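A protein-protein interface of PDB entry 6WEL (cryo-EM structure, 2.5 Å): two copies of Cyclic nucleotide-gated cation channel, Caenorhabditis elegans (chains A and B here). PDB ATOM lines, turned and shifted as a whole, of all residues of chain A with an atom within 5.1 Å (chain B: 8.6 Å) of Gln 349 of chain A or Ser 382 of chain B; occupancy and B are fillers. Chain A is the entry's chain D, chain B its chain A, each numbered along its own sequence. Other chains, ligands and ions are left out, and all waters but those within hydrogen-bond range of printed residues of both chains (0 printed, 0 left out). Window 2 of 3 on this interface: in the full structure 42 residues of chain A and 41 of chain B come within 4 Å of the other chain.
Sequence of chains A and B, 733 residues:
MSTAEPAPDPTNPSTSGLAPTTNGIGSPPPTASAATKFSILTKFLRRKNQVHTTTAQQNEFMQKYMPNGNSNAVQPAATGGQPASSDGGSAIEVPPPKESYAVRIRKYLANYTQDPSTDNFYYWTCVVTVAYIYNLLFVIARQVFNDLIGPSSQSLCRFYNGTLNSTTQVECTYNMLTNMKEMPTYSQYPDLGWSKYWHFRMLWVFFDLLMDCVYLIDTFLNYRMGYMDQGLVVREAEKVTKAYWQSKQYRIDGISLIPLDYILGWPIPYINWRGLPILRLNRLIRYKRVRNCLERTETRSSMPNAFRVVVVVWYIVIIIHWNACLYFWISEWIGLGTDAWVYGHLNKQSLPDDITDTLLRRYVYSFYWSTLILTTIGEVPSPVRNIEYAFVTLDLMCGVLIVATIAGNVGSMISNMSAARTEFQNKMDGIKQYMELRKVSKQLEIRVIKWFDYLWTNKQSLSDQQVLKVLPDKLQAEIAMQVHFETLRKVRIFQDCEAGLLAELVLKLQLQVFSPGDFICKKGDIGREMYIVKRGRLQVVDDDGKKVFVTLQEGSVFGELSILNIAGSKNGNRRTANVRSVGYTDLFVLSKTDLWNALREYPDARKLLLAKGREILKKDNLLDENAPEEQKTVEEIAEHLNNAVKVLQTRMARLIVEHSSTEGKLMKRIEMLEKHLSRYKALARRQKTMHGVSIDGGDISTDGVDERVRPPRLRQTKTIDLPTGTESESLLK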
ATOM      1  N   ASN A 347      22.581   2.804 -21.963  1.00  0.00           N
ATOM      2  CA  ASN A 347      22.966   4.180 -22.235  1.00  0.00           C
ATOM      3  C   ASN A 347      21.743   4.825 -22.867  1.00  0.00           C
ATOM      4  O   ASN A 347      21.395   4.534 -24.008  1.00  0.00           O
ATOM      5  CB  ASN A 347      24.197   4.212 -23.131  1.00  0.00           C
ATOM      6  CG  ASN A 347      24.754   5.581 -23.320  1.00  0.00           C
ATOM      7  OD1 ASN A 347      24.114   6.565 -23.022  1.00  0.00           O
ATOM      8  ND2 ASN A 347      25.948   5.654 -23.841  1.00  0.00           N
ATOM      9  N   LYS A 348      21.055   5.660 -22.100  1.00  0.00           N
ATOM     10  CA  LYS A 348      19.813   6.288 -22.519  1.00  0.00           C
ATOM     11  C   LYS A 348      20.035   7.543 -23.338  1.00  0.00           C
ATOM     12  O   LYS A 348      19.066   8.165 -23.766  1.00  0.00           O
ATOM     13  CB  LYS A 348      18.964   6.614 -21.298  1.00  0.00           C
ATOM     14  CG  LYS A 348      17.828   5.674 -21.070  1.00  0.00           C
ATOM     15  CD  LYS A 348      18.298   4.311 -20.678  1.00  0.00           C
ATOM     16  CE  LYS A 348      17.175   3.303 -20.811  1.00  0.00           C
ATOM     17  NZ  LYS A 348      17.618   1.909 -20.541  1.00  0.00           N
ATOM     18  N   GLN A 349      21.277   7.948 -23.530  1.00  0.00           N
ATOM     19  CA  GLN A 349      21.610   8.929 -24.542  1.00  0.00           C
ATOM     20  C   GLN A 349      21.870   8.264 -25.882  1.00  0.00           C
ATOM     21  O   GLN A 349      21.515   8.826 -26.918  1.00  0.00           O
ATOM     22  CB  GLN A 349      22.826   9.738 -24.090  1.00  0.00           C
ATOM     23  CG  GLN A 349      22.947  11.111 -24.689  1.00  0.00           C
ATOM     24  CD  GLN A 349      24.280  11.736 -24.409  1.00  0.00           C
ATOM     25  OE1 GLN A 349      25.243  11.043 -24.171  1.00  0.00           O
ATOM     26  NE2 GLN A 349      24.347  13.045 -24.439  1.00  0.00           N
ATOM     27  N   SER A 350      22.476   7.074 -25.873  1.00  0.00           N
ATOM     28  CA  SER A 350      22.598   6.252 -27.071  1.00  0.00           C
ATOM     29  C   SER A 350      21.244   5.973 -27.677  1.00  0.00           C
ATOM     30  O   SER A 350      20.976   6.304 -28.833  1.00  0.00           O
ATOM     31  CB  SER A 350      23.260   4.924 -26.734  1.00  0.00           C
ATOM     32  OG  SER A 350      24.645   5.009 -26.790  1.00  0.00           O
ATOM     33  N   LEU A 351      20.387   5.320 -26.905  1.00  0.00           N
ATOM     34  CA  LEU A 351      19.103   4.827 -27.377  1.00  0.00           C
ATOM     35  C   LEU A 351      18.021   5.394 -26.477  1.00  0.00           C
ATOM     36  O   LEU A 351      17.616   4.742 -25.504  1.00  0.00           O
ATOM     37  CB  LEU A 351      19.086   3.306 -27.393  1.00  0.00           C
ATOM     38  CG  LEU A 351      20.038   2.726 -28.445  1.00  0.00           C
ATOM     39  CD1 LEU A 351      20.204   1.246 -28.314  1.00  0.00           C
ATOM     40  CD2 LEU A 351      19.544   3.077 -29.821  1.00  0.00           C
ATOM     41  N   PRO A 352      17.534   6.591 -26.771  1.00  0.00           N
ATOM     42  CA  PRO A 352      16.387   7.139 -26.048  1.00  0.00           C
ATOM     43  C   PRO A 352      15.104   6.409 -26.381  1.00  0.00           C
ATOM     44  O   PRO A 352      15.127   5.307 -26.932  1.00  0.00           O
ATOM     45  CB  PRO A 352      16.334   8.590 -26.526  1.00  0.00           C
ATOM     46  CG  PRO A 352      17.633   8.871 -27.033  1.00  0.00           C
ATOM     47  CD  PRO A 352      18.163   7.618 -27.603  1.00  0.00           C
ATOM     48  N   ARG A 361      22.614   5.007 -36.525  1.00  0.00           N
ATOM     49  CA  ARG A 361      22.564   5.469 -35.142  1.00  0.00           C
ATOM     50  C   ARG A 361      23.866   5.187 -34.407  1.00  0.00           C
ATOM     51  O   ARG A 361      24.333   6.025 -33.636  1.00  0.00           O
ATOM     52  CB  ARG A 361      21.392   4.824 -34.409  1.00  0.00           C
ATOM     53  CG  ARG A 361      21.227   5.258 -32.979  1.00  0.00           C
ATOM     54  CD  ARG A 361      21.043   6.733 -32.898  1.00  0.00           C
ATOM     55  NE  ARG A 361      20.740   7.206 -31.559  1.00  0.00           N
ATOM     56  CZ  ARG A 361      20.192   8.385 -31.307  1.00  0.00           C
ATOM     57  NH1 ARG A 361      19.887   9.185 -32.299  1.00  0.00           N
ATOM     58  NH2 ARG A 361      19.936   8.760 -30.073  1.00  0.00           N
ATOM     59  N   TYR A 365      25.876   8.386 -32.970  1.00  0.00           N
ATOM     60  CA  TYR A 365      26.131   8.549 -31.549  1.00  0.00           C
ATOM     61  C   TYR A 365      27.617   8.498 -31.235  1.00  0.00           C
ATOM     62  O   TYR A 365      28.089   9.252 -30.386  1.00  0.00           O
ATOM     63  CB  TYR A 365      25.388   7.502 -30.727  1.00  0.00           C
ATOM     64  CG  TYR A 365      25.661   7.712 -29.267  1.00  0.00           C
ATOM     65  CD1 TYR A 365      25.030   8.721 -28.575  1.00  0.00           C
ATOM     66  CD2 TYR A 365      26.595   6.949 -28.591  1.00  0.00           C
ATOM     67  CE1 TYR A 365      25.299   8.945 -27.270  1.00  0.00           C
ATOM     68  CE2 TYR A 365      26.862   7.173 -27.280  1.00  0.00           C
ATOM     69  CZ  TYR A 365      26.210   8.175 -26.626  1.00  0.00           C
ATOM     70  OH  TYR A 365      26.460   8.415 -25.310  1.00  0.00           O
ATOM     71  N   TYR A 368      29.095  11.881 -32.142  1.00  0.00           N
ATOM     72  CA  TYR A 368      28.737  12.907 -31.170  1.00  0.00           C
ATOM     73  C   TYR A 368      29.493  12.732 -29.855  1.00  0.00           C
ATOM     74  O   TYR A 368      29.982  13.707 -29.273  1.00  0.00           O
ATOM     75  CB  TYR A 368      27.229  12.877 -30.946  1.00  0.00           C
ATOM     76  CG  TYR A 368      26.706  13.824 -29.899  1.00  0.00           C
ATOM     77  CD1 TYR A 368      26.453  15.147 -30.204  1.00  0.00           C
ATOM     78  CD2 TYR A 368      26.447  13.388 -28.607  1.00  0.00           C
ATOM     79  CE1 TYR A 368      25.978  15.996 -29.264  1.00  0.00           C
ATOM     80  CE2 TYR A 368      25.977  14.234 -27.669  1.00  0.00           C
ATOM     81  CZ  TYR A 368      25.740  15.534 -27.999  1.00  0.00           C
ATOM     82  OH  TYR A 368      25.258  16.388 -27.054  1.00  0.00           O
ATOM     83  N   GLU A 379      29.556  16.364 -22.070  1.00  0.00           N
ATOM     84  CA  GLU A 379      28.161  16.151 -21.704  1.00  0.00           C
ATOM     85  C   GLU A 379      27.683  14.773 -22.128  1.00  0.00           C
ATOM     86  O   GLU A 379      26.695  14.621 -22.830  1.00  0.00           O
ATOM     87  CB  GLU A 379      27.298  17.237 -22.319  1.00  0.00           C
ATOM     88  CG  GLU A 379      27.695  18.620 -21.938  1.00  0.00           C
ATOM     89  CD  GLU A 379      27.259  18.964 -20.557  1.00  0.00           C
ATOM     90  OE1 GLU A 379      26.192  18.483 -20.143  1.00  0.00           O
ATOM     91  OE2 GLU A 379      27.985  19.713 -19.882  1.00  0.00           O
ATOM     92  N   VAL A 380      28.413  13.758 -21.694  1.00  0.00           N
ATOM     93  CA  VAL A 380      28.139  12.365 -22.025  1.00  0.00           C
ATOM     94  C   VAL A 380      28.117  11.587 -20.717  1.00  0.00           C
ATOM     95  O   VAL A 380      28.560  12.096 -19.680  1.00  0.00           O
ATOM     96  CB  VAL A 380      29.188  11.797 -23.009  1.00  0.00           C
ATOM     97  CG1 VAL A 380      28.987  12.363 -24.400  1.00  0.00           C
ATOM     98  CG2 VAL A 380      30.570  12.111 -22.541  1.00  0.00           C
ATOM     99  N   PRO A 381      27.579  10.369 -20.723  1.00  0.00           N
ATOM    100  CA  PRO A 381      27.596   9.561 -19.504  1.00  0.00           C
ATOM    101  C   PRO A 381      28.998   9.349 -18.955  1.00  0.00           C
ATOM    102  O   PRO A 381      29.970   9.225 -19.694  1.00  0.00           O
ATOM    103  CB  PRO A 381      26.972   8.245 -19.962  1.00  0.00           C
ATOM    104  CG  PRO A 381      26.067   8.645 -21.003  1.00  0.00           C
ATOM    105  CD  PRO A 381      26.711   9.760 -21.739  1.00  0.00           C
ATOM    106  N   TYR B 327      17.632  27.454 -34.313  1.00  0.00           N
ATOM    107  CA  TYR B 327      17.175  26.456 -33.358  1.00  0.00           C
ATOM    108  C   TYR B 327      15.663  26.395 -33.304  1.00  0.00           C
ATOM    109  O   TYR B 327      15.080  25.309 -33.295  1.00  0.00           O
ATOM    110  CB  TYR B 327      17.727  26.739 -31.961  1.00  0.00           C
ATOM    111  CG  TYR B 327      17.090  25.863 -30.903  1.00  0.00           C
ATOM    112  CD1 TYR B 327      17.394  24.523 -30.829  1.00  0.00           C
ATOM    113  CD2 TYR B 327      16.168  26.369 -30.003  1.00  0.00           C
ATOM    114  CE1 TYR B 327      16.824  23.723 -29.904  1.00  0.00           C
ATOM    115  CE2 TYR B 327      15.588  25.567 -29.081  1.00  0.00           C
ATOM    116  CZ  TYR B 327      15.928  24.238 -29.040  1.00  0.00           C
ATOM    117  OH  TYR B 327      15.383  23.399 -28.123  1.00  0.00           O
ATOM    118  N   ASP B 339       9.858  15.838 -28.779  1.00  0.00           N
ATOM    119  CA  ASP B 339      10.861  15.160 -27.980  1.00  0.00           C
ATOM    120  C   ASP B 339      11.371  16.140 -26.934  1.00  0.00           C
ATOM    121  O   ASP B 339      10.847  17.241 -26.784  1.00  0.00           O
ATOM    122  CB  ASP B 339      11.976  14.559 -28.850  1.00  0.00           C
ATOM    123  CG  ASP B 339      12.616  15.552 -29.782  1.00  0.00           C
ATOM    124  OD1 ASP B 339      13.253  16.493 -29.308  1.00  0.00           O
ATOM    125  OD2 ASP B 339      12.514  15.372 -31.001  1.00  0.00           O
ATOM    126  N   ALA B 340      12.385  15.725 -26.190  1.00  0.00           N
ATOM    127  CA  ALA B 340      12.906  16.489 -25.072  1.00  0.00           C
ATOM    128  C   ALA B 340      14.006  17.450 -25.466  1.00  0.00           C
ATOM    129  O   ALA B 340      14.621  18.050 -24.589  1.00  0.00           O
ATOM    130  CB  ALA B 340      13.416  15.546 -23.993  1.00  0.00           C
ATOM    131  N   TRP B 341      14.275  17.602 -26.753  1.00  0.00           N
ATOM    132  CA  TRP B 341      15.281  18.522 -27.250  1.00  0.00           C
ATOM    133  C   TRP B 341      14.680  19.760 -27.887  1.00  0.00           C
ATOM    134  O   TRP B 341      15.212  20.853 -27.717  1.00  0.00           O
ATOM    135  CB  TRP B 341      16.192  17.807 -28.251  1.00  0.00           C
ATOM    136  CG  TRP B 341      17.232  18.669 -28.879  1.00  0.00           C
ATOM    137  CD1 TRP B 341      18.466  18.916 -28.407  1.00  0.00           C
ATOM    138  CD2 TRP B 341      17.123  19.395 -30.103  1.00  0.00           C
ATOM    139  NE1 TRP B 341      19.138  19.745 -29.245  1.00  0.00           N
ATOM    140  CE2 TRP B 341      18.327  20.057 -30.298  1.00  0.00           C
ATOM    141  CE3 TRP B 341      16.112  19.557 -31.048  1.00  0.00           C
ATOM    142  CZ2 TRP B 341      18.553  20.858 -31.391  1.00  0.00           C
ATOM    143  CZ3 TRP B 341      16.336  20.345 -32.120  1.00  0.00           C
ATOM    144  CH2 TRP B 341      17.544  20.984 -32.295  1.00  0.00           C
ATOM    145  N   VAL B 342      13.567  19.618 -28.597  1.00  0.00           N
ATOM    146  CA  VAL B 342      12.919  20.762 -29.201  1.00  0.00           C
ATOM    147  C   VAL B 342      12.212  21.587 -28.131  1.00  0.00           C
ATOM    148  O   VAL B 342      11.849  21.093 -27.061  1.00  0.00           O
ATOM    149  CB  VAL B 342      11.942  20.317 -30.303  1.00  0.00           C
ATOM    150  CG1 VAL B 342      12.672  19.658 -31.414  1.00  0.00           C
ATOM    151  CG2 VAL B 342      10.926  19.385 -29.768  1.00  0.00           C
ATOM    152  N   ASN B 347      10.447  19.319 -23.231  1.00  0.00           N
ATOM    153  CA  ASN B 347      11.688  19.960 -22.827  1.00  0.00           C
ATOM    154  C   ASN B 347      11.349  20.741 -21.566  1.00  0.00           C
ATOM    155  O   ASN B 347      10.660  21.757 -21.619  1.00  0.00           O
ATOM    156  CB  ASN B 347      12.216  20.836 -23.954  1.00  0.00           C
ATOM    157  CG  ASN B 347      13.571  21.396 -23.681  1.00  0.00           C
ATOM    158  OD1 ASN B 347      14.044  21.379 -22.567  1.00  0.00           O
ATOM    159  ND2 ASN B 347      14.196  21.922 -24.699  1.00  0.00           N
ATOM    160  N   GLN B 349      13.385  22.236 -19.558  1.00  0.00           N
ATOM    161  CA  GLN B 349      14.117  23.480 -19.445  1.00  0.00           C
ATOM    162  C   GLN B 349      13.439  24.586 -20.234  1.00  0.00           C
ATOM    163  O   GLN B 349      13.441  25.735 -19.794  1.00  0.00           O
ATOM    164  CB  GLN B 349      15.554  23.273 -19.923  1.00  0.00           C
ATOM    165  CG  GLN B 349      16.567  24.227 -19.354  1.00  0.00           C
ATOM    166  CD  GLN B 349      17.889  24.135 -20.056  1.00  0.00           C
ATOM    167  OE1 GLN B 349      17.951  23.720 -21.190  1.00  0.00           O
ATOM    168  NE2 GLN B 349      18.948  24.525 -19.390  1.00  0.00           N
ATOM    169  N   TYR B 365      14.225  31.450 -24.542  1.00  0.00           N
ATOM    170  CA  TYR B 365      14.823  30.130 -24.440  1.00  0.00           C
ATOM    171  C   TYR B 365      15.709  29.820 -25.635  1.00  0.00           C
ATOM    172  O   TYR B 365      16.766  29.213 -25.474  1.00  0.00           O
ATOM    173  CB  TYR B 365      13.760  29.049 -24.285  1.00  0.00           C
ATOM    174  CG  TYR B 365      14.415  27.704 -24.165  1.00  0.00           C
ATOM    175  CD1 TYR B 365      15.002  27.314 -22.984  1.00  0.00           C
ATOM    176  CD2 TYR B 365      14.505  26.849 -25.247  1.00  0.00           C
ATOM    177  CE1 TYR B 365      15.630  26.122 -22.877  1.00  0.00           C
ATOM    178  CE2 TYR B 365      15.134  25.650 -25.138  1.00  0.00           C
ATOM    179  CZ  TYR B 365      15.694  25.295 -23.949  1.00  0.00           C
ATOM    180  OH  TYR B 365      16.326  24.097 -23.817  1.00  0.00           O
ATOM    181  N   TRP B 369      19.624  28.857 -25.299  1.00  0.00           N
ATOM    182  CA  TRP B 369      20.119  27.635 -25.912  1.00  0.00           C
ATOM    183  C   TRP B 369      21.288  27.923 -26.839  1.00  0.00           C
ATOM    184  O   TRP B 369      22.325  27.254 -26.785  1.00  0.00           O
ATOM    185  CB  TRP B 369      18.980  26.943 -26.674  1.00  0.00           C
ATOM    186  CG  TRP B 369      19.326  25.572 -27.133  1.00  0.00           C
ATOM    187  CD1 TRP B 369      19.088  24.422 -26.479  1.00  0.00           C
ATOM    188  CD2 TRP B 369      20.008  25.213 -28.336  1.00  0.00           C
ATOM    189  NE1 TRP B 369      19.565  23.366 -27.185  1.00  0.00           N
ATOM    190  CE2 TRP B 369      20.140  23.827 -28.336  1.00  0.00           C
ATOM    191  CE3 TRP B 369      20.514  25.936 -29.422  1.00  0.00           C
ATOM    192  CZ2 TRP B 369      20.755  23.144 -29.370  1.00  0.00           C
ATOM    193  CZ3 TRP B 369      21.120  25.262 -30.432  1.00  0.00           C
ATOM    194  CH2 TRP B 369      21.235  23.876 -30.405  1.00  0.00           C
ATOM    195  N   ILE B 373      25.265  26.801 -26.583  1.00  0.00           N
ATOM    196  CA  ILE B 373      25.840  25.911 -27.583  1.00  0.00           C
ATOM    197  C   ILE B 373      27.017  26.561 -28.297  1.00  0.00           C
ATOM    198  O   ILE B 373      28.035  25.914 -28.546  1.00  0.00           O
ATOM    199  CB  ILE B 373      24.744  25.459 -28.558  1.00  0.00           C
ATOM    200  CG1 ILE B 373      23.863  24.409 -27.890  1.00  0.00           C
ATOM    201  CG2 ILE B 373      25.332  24.934 -29.837  1.00  0.00           C
ATOM    202  CD1 ILE B 373      24.540  23.134 -27.582  1.00  0.00           C
ATOM    203  N   GLY B 378      27.194  24.055 -23.137  1.00  0.00           N
ATOM    204  CA  GLY B 378      26.489  22.822 -23.404  1.00  0.00           C
ATOM    205  C   GLY B 378      25.614  22.307 -22.293  1.00  0.00           C
ATOM    206  O   GLY B 378      25.400  21.102 -22.201  1.00  0.00           O
ATOM    207  N   GLU B 379      25.090  23.181 -21.448  1.00  0.00           N
ATOM    208  CA  GLU B 379      24.205  22.765 -20.368  1.00  0.00           C
ATOM    209  C   GLU B 379      22.751  22.792 -20.805  1.00  0.00           C
ATOM    210  O   GLU B 379      21.904  23.421 -20.190  1.00  0.00           O
ATOM    211  CB  GLU B 379      24.422  23.652 -19.156  1.00  0.00           C
ATOM    212  CG  GLU B 379      25.824  23.668 -18.656  1.00  0.00           C
ATOM    213  CD  GLU B 379      26.158  22.433 -17.895  1.00  0.00           C
ATOM    214  OE1 GLU B 379      25.261  21.899 -17.224  1.00  0.00           O
ATOM    215  OE2 GLU B 379      27.319  21.994 -17.970  1.00  0.00           O
ATOM    216  N   VAL B 380      22.471  22.099 -21.897  1.00  0.00           N
ATOM    217  CA  VAL B 380      21.143  22.032 -22.495  1.00  0.00           C
ATOM    218  C   VAL B 380      20.816  20.561 -22.706  1.00  0.00           C
ATOM    219  O   VAL B 380      21.708  19.706 -22.626  1.00  0.00           O
ATOM    220  CB  VAL B 380      21.076  22.827 -23.820  1.00  0.00           C
ATOM    221  CG1 VAL B 380      21.089  24.319 -23.558  1.00  0.00           C
ATOM    222  CG2 VAL B 380      22.224  22.470 -24.706  1.00  0.00           C
ATOM    223  N   PRO B 381      19.549  20.229 -22.940  1.00  0.00           N
ATOM    224  CA  PRO B 381      19.201  18.835 -23.212  1.00  0.00           C
ATOM    225  C   PRO B 381      19.965  18.254 -24.392  1.00  0.00           C
ATOM    226  O   PRO B 381      20.258  18.935 -25.371  1.00  0.00           O
ATOM    227  CB  PRO B 381      17.703  18.911 -23.502  1.00  0.00           C
ATOM    228  CG  PRO B 381      17.260  20.017 -22.700  1.00  0.00           C
ATOM    229  CD  PRO B 381      18.340  21.035 -22.725  1.00  0.00           C
ATOM    230  N   SER B 382      20.283  16.970 -24.285  1.00  0.00           N
ATOM    231  CA  SER B 382      20.968  16.273 -25.356  1.00  0.00           C
ATOM    232  C   SER B 382      20.010  16.018 -26.513  1.00  0.00           C
ATOM    233  O   SER B 382      18.802  15.912 -26.308  1.00  0.00           O
ATOM    234  CB  SER B 382      21.522  14.949 -24.860  1.00  0.00           C
ATOM    235  OG  SER B 382      21.715  14.977 -23.470  1.00  0.00           O
ATOM    236  N   PRO B 383      20.524  15.904 -27.733  1.00  0.00           N
ATOM    237  CA  PRO B 383      19.655  15.599 -28.864  1.00  0.00           C
ATOM    238  C   PRO B 383      19.063  14.214 -28.727  1.00  0.00           C
ATOM    239  O   PRO B 383      19.534  13.377 -27.961  1.00  0.00           O
ATOM    240  CB  PRO B 383      20.591  15.683 -30.064  1.00  0.00           C
ATOM    241  CG  PRO B 383      21.815  16.279 -29.574  1.00  0.00           C
ATOM    242  CD  PRO B 383      21.925  16.008 -28.152  1.00  0.00           C
ATOM    243  N   VAL B 384      18.000  13.972 -29.476  1.00  0.00           N
ATOM    244  CA  VAL B 384      17.255  12.725 -29.397  1.00  0.00           C
ATOM    245  C   VAL B 384      17.271  11.980 -30.725  1.00  0.00           C
ATOM    246  O   VAL B 384      17.523  10.780 -30.768  1.00  0.00           O
ATOM    247  CB  VAL B 384      15.808  12.963 -28.917  1.00  0.00           C
ATOM    248  CG1 VAL B 384      15.085  11.671 -28.794  1.00  0.00           C
ATOM    249  CG2 VAL B 384      15.805  13.683 -27.598  1.00  0.00           C
ATOM    250  N   ARG B 385      17.042  12.688 -31.817  1.00  0.00           N
ATOM    251  CA  ARG B 385      16.975  12.108 -33.146  1.00  0.00           C
ATOM    252  C   ARG B 385      18.271  12.340 -33.905  1.00  0.00           C
ATOM    253  O   ARG B 385      19.099  13.157 -33.516  1.00  0.00           O
ATOM    254  CB  ARG B 385      15.800  12.698 -33.903  1.00  0.00           C
ATOM    255  CG  ARG B 385      14.538  12.598 -33.130  1.00  0.00           C
ATOM    256  CD  ARG B 385      13.410  13.221 -33.858  1.00  0.00           C
ATOM    257  NE  ARG B 385      13.170  12.568 -35.126  1.00  0.00           N
ATOM    258  CZ  ARG B 385      12.142  12.838 -35.914  1.00  0.00           C
ATOM    259  NH1 ARG B 385      11.254  13.746 -35.559  1.00  0.00           N
ATOM    260  NH2 ARG B 385      12.003  12.194 -37.057  1.00  0.00           N
ATOM    261  N   ASN B 386      18.444  11.597 -34.997  1.00  0.00           N
ATOM    262  CA  ASN B 386      19.678  11.681 -35.771  1.00  0.00           C
ATOM    263  C   ASN B 386      19.860  13.059 -36.382  1.00  0.00           C
ATOM    264  O   ASN B 386      20.983  13.556 -36.488  1.00  0.00           O
ATOM    265  CB  ASN B 386      19.692  10.617 -36.865  1.00  0.00           C
ATOM    266  CG  ASN B 386      19.917   9.234 -36.333  1.00  0.00           C
ATOM    267  OD1 ASN B 386      20.571   9.049 -35.331  1.00  0.00           O
ATOM    268  ND2 ASN B 386      19.383   8.251 -37.016  1.00  0.00           N
ATOM    269  N   GLU B 388      18.763  15.893 -35.120  1.00  0.00           N
ATOM    270  CA  GLU B 388      19.167  16.780 -34.040  1.00  0.00           C
ATOM    271  C   GLU B 388      20.621  16.560 -33.664  1.00  0.00           C
ATOM    272  O   GLU B 388      21.333  17.513 -33.357  1.00  0.00           O
ATOM    273  CB  GLU B 388      18.268  16.570 -32.837  1.00  0.00           C
ATOM    274  CG  GLU B 388      16.820  16.708 -33.147  1.00  0.00           C
ATOM    275  CD  GLU B 388      15.972  16.291 -32.004  1.00  0.00           C
ATOM    276  OE1 GLU B 388      16.534  15.807 -31.028  1.00  0.00           O
ATOM    277  OE2 GLU B 388      14.753  16.431 -32.068  1.00  0.00           O
ATOM    278  N   TYR B 389      21.078  15.309 -33.688  1.00  0.00           N
ATOM    279  CA  TYR B 389      22.488  15.009 -33.463  1.00  0.00           C
ATOM    280  C   TYR B 389      23.366  15.685 -34.494  1.00  0.00           C
ATOM    281  O   TYR B 389      24.402  16.256 -34.156  1.00  0.00           O
ATOM    282  CB  TYR B 389      22.712  13.500 -33.483  1.00  0.00           C
ATOM    283  CG  TYR B 389      22.565  12.871 -32.137  1.00  0.00           C
ATOM    284  CD1 TYR B 389      23.633  12.783 -31.283  1.00  0.00           C
ATOM    285  CD2 TYR B 389      21.358  12.391 -31.709  1.00  0.00           C
ATOM    286  CE1 TYR B 389      23.502  12.231 -30.057  1.00  0.00           C
ATOM    287  CE2 TYR B 389      21.227  11.841 -30.483  1.00  0.00           C
ATOM    288  CZ  TYR B 389      22.300  11.767 -29.658  1.00  0.00           C
ATOM    289  OH  TYR B 389      22.179  11.212 -28.419  1.00  0.00           O
ATOM    290  N   VAL B 392      23.386  19.504 -33.863  1.00  0.00           N
ATOM    291  CA  VAL B 392      24.096  19.901 -32.655  1.00  0.00           C
ATOM    292  C   VAL B 392      25.591  19.652 -32.793  1.00  0.00           C
ATOM    293  O   VAL B 392      26.400  20.431 -32.296  1.00  0.00           O
ATOM    294  CB  VAL B 392      23.505  19.190 -31.429  1.00  0.00           C
ATOM    295  CG1 VAL B 392      24.284  19.537 -30.208  1.00  0.00           C
ATOM    296  CG2 VAL B 392      22.098  19.606 -31.239  1.00  0.00           C
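The side-chain hydroxyl of Ser 382 of chain B lies within hydrogen-bond range of the side-chain amide nitrogen of Gln 349 of chain A.
The backbone carbonyl oxygen of Val 384 of chain B is in hydrogen-bond range of the guanidinium group of Arg 361 of chain A, at 3.2 Å.
The guanidinium group (NH1) of Arg 361 of chain A is in hydrogen-bond range of the side-chain amide oxygen (OD1) of Asn 386 of chain B (3.1 Å).
The backbone carbonyl oxygen (O) of Gln 349 of chain A is in hydrogen-bond range of the side-chain hydroxyl (OH) of Tyr 389 of chain B.
The side-chain carboxylate (OE1) of Glu 379 of chain A lies close to the backbone carbonyl oxygen (O) of Gly 378 of chain B.
The side-chain carboxylate (OE2) of Glu 379 of chain A lies close to the side-chain carboxylate (OE2) of Glu 379 of chain B.
The side-chain hydroxyl (OH) of Tyr 365 of chain A sits at hydrogen-bond distance from the side-chain amide nitrogen (ND2) of Asn 347 of chain A (3.2 Å).
The backbone carbonyl oxygen of Glu 379 of chain A sits at hydrogen-bond distance from the side-chain amide nitrogen of Gln 349 of chain A (3.3 Å).
Among the printed residues, merely in contact across the chains: Arg 361 of chain A with Tyr 389 of chain B, Tyr 368 of chain A with Tyr 389 of chain B, Tyr 368 of chain A with Pro 383 of chain B, Tyr 365 of chain A with Tyr 389 of chain B and Arg 361 of chain A with Arg 385 of chain B.
Of chain B, only Ser 382 and Tyr 389 come within 4 Å of Gln 349 of chain A.
Of chain A, only Gln 349 (3.4 Å) comes within 4 Å of Ser 382 of chain B.
No residue of chain B comes within 4 Å of Ser 350 of chain A.
Printed residues of chain B within 4 Å of Tyr 368 of chain A: Pro 383 (3.5 Å) and Tyr 389 (3.5 Å).
Of the printed residues of chain A, Arg 385 of chain B touches Arg 361 (3.9 Å).
Gln 349 of chain B touches none of the printed residues of chain A.
Val 380 of chain A touches none of the printed residues of chain B.
The nearest printed residue of chain B that does not touch Tyr 368 of chain A is Val 392 of chain B (4.04 Å).
Of the 22 printed residues of chain B, 8 touch a printed residue of chain A.
Of the 12 printed residues of chain A, 5 touch a printed residue of chain B.
Hydrophobic or aromatic side chains of chain A within 4 Å of the printed part of chain B: Tyr 365 and Tyr 368.
Among the printed residues, 11 pairs touch across the chains.
Among the printed residues, no Asp or Glu carboxylate lies within 4 Å of a Lys or Arg side-chain nitrogen of the other chain.
Glu 379 of chain B touches its own counterpart, Glu 379 of chain A.
Positions printed for both chains: 347, 349, 365, 379, 380 and 381.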
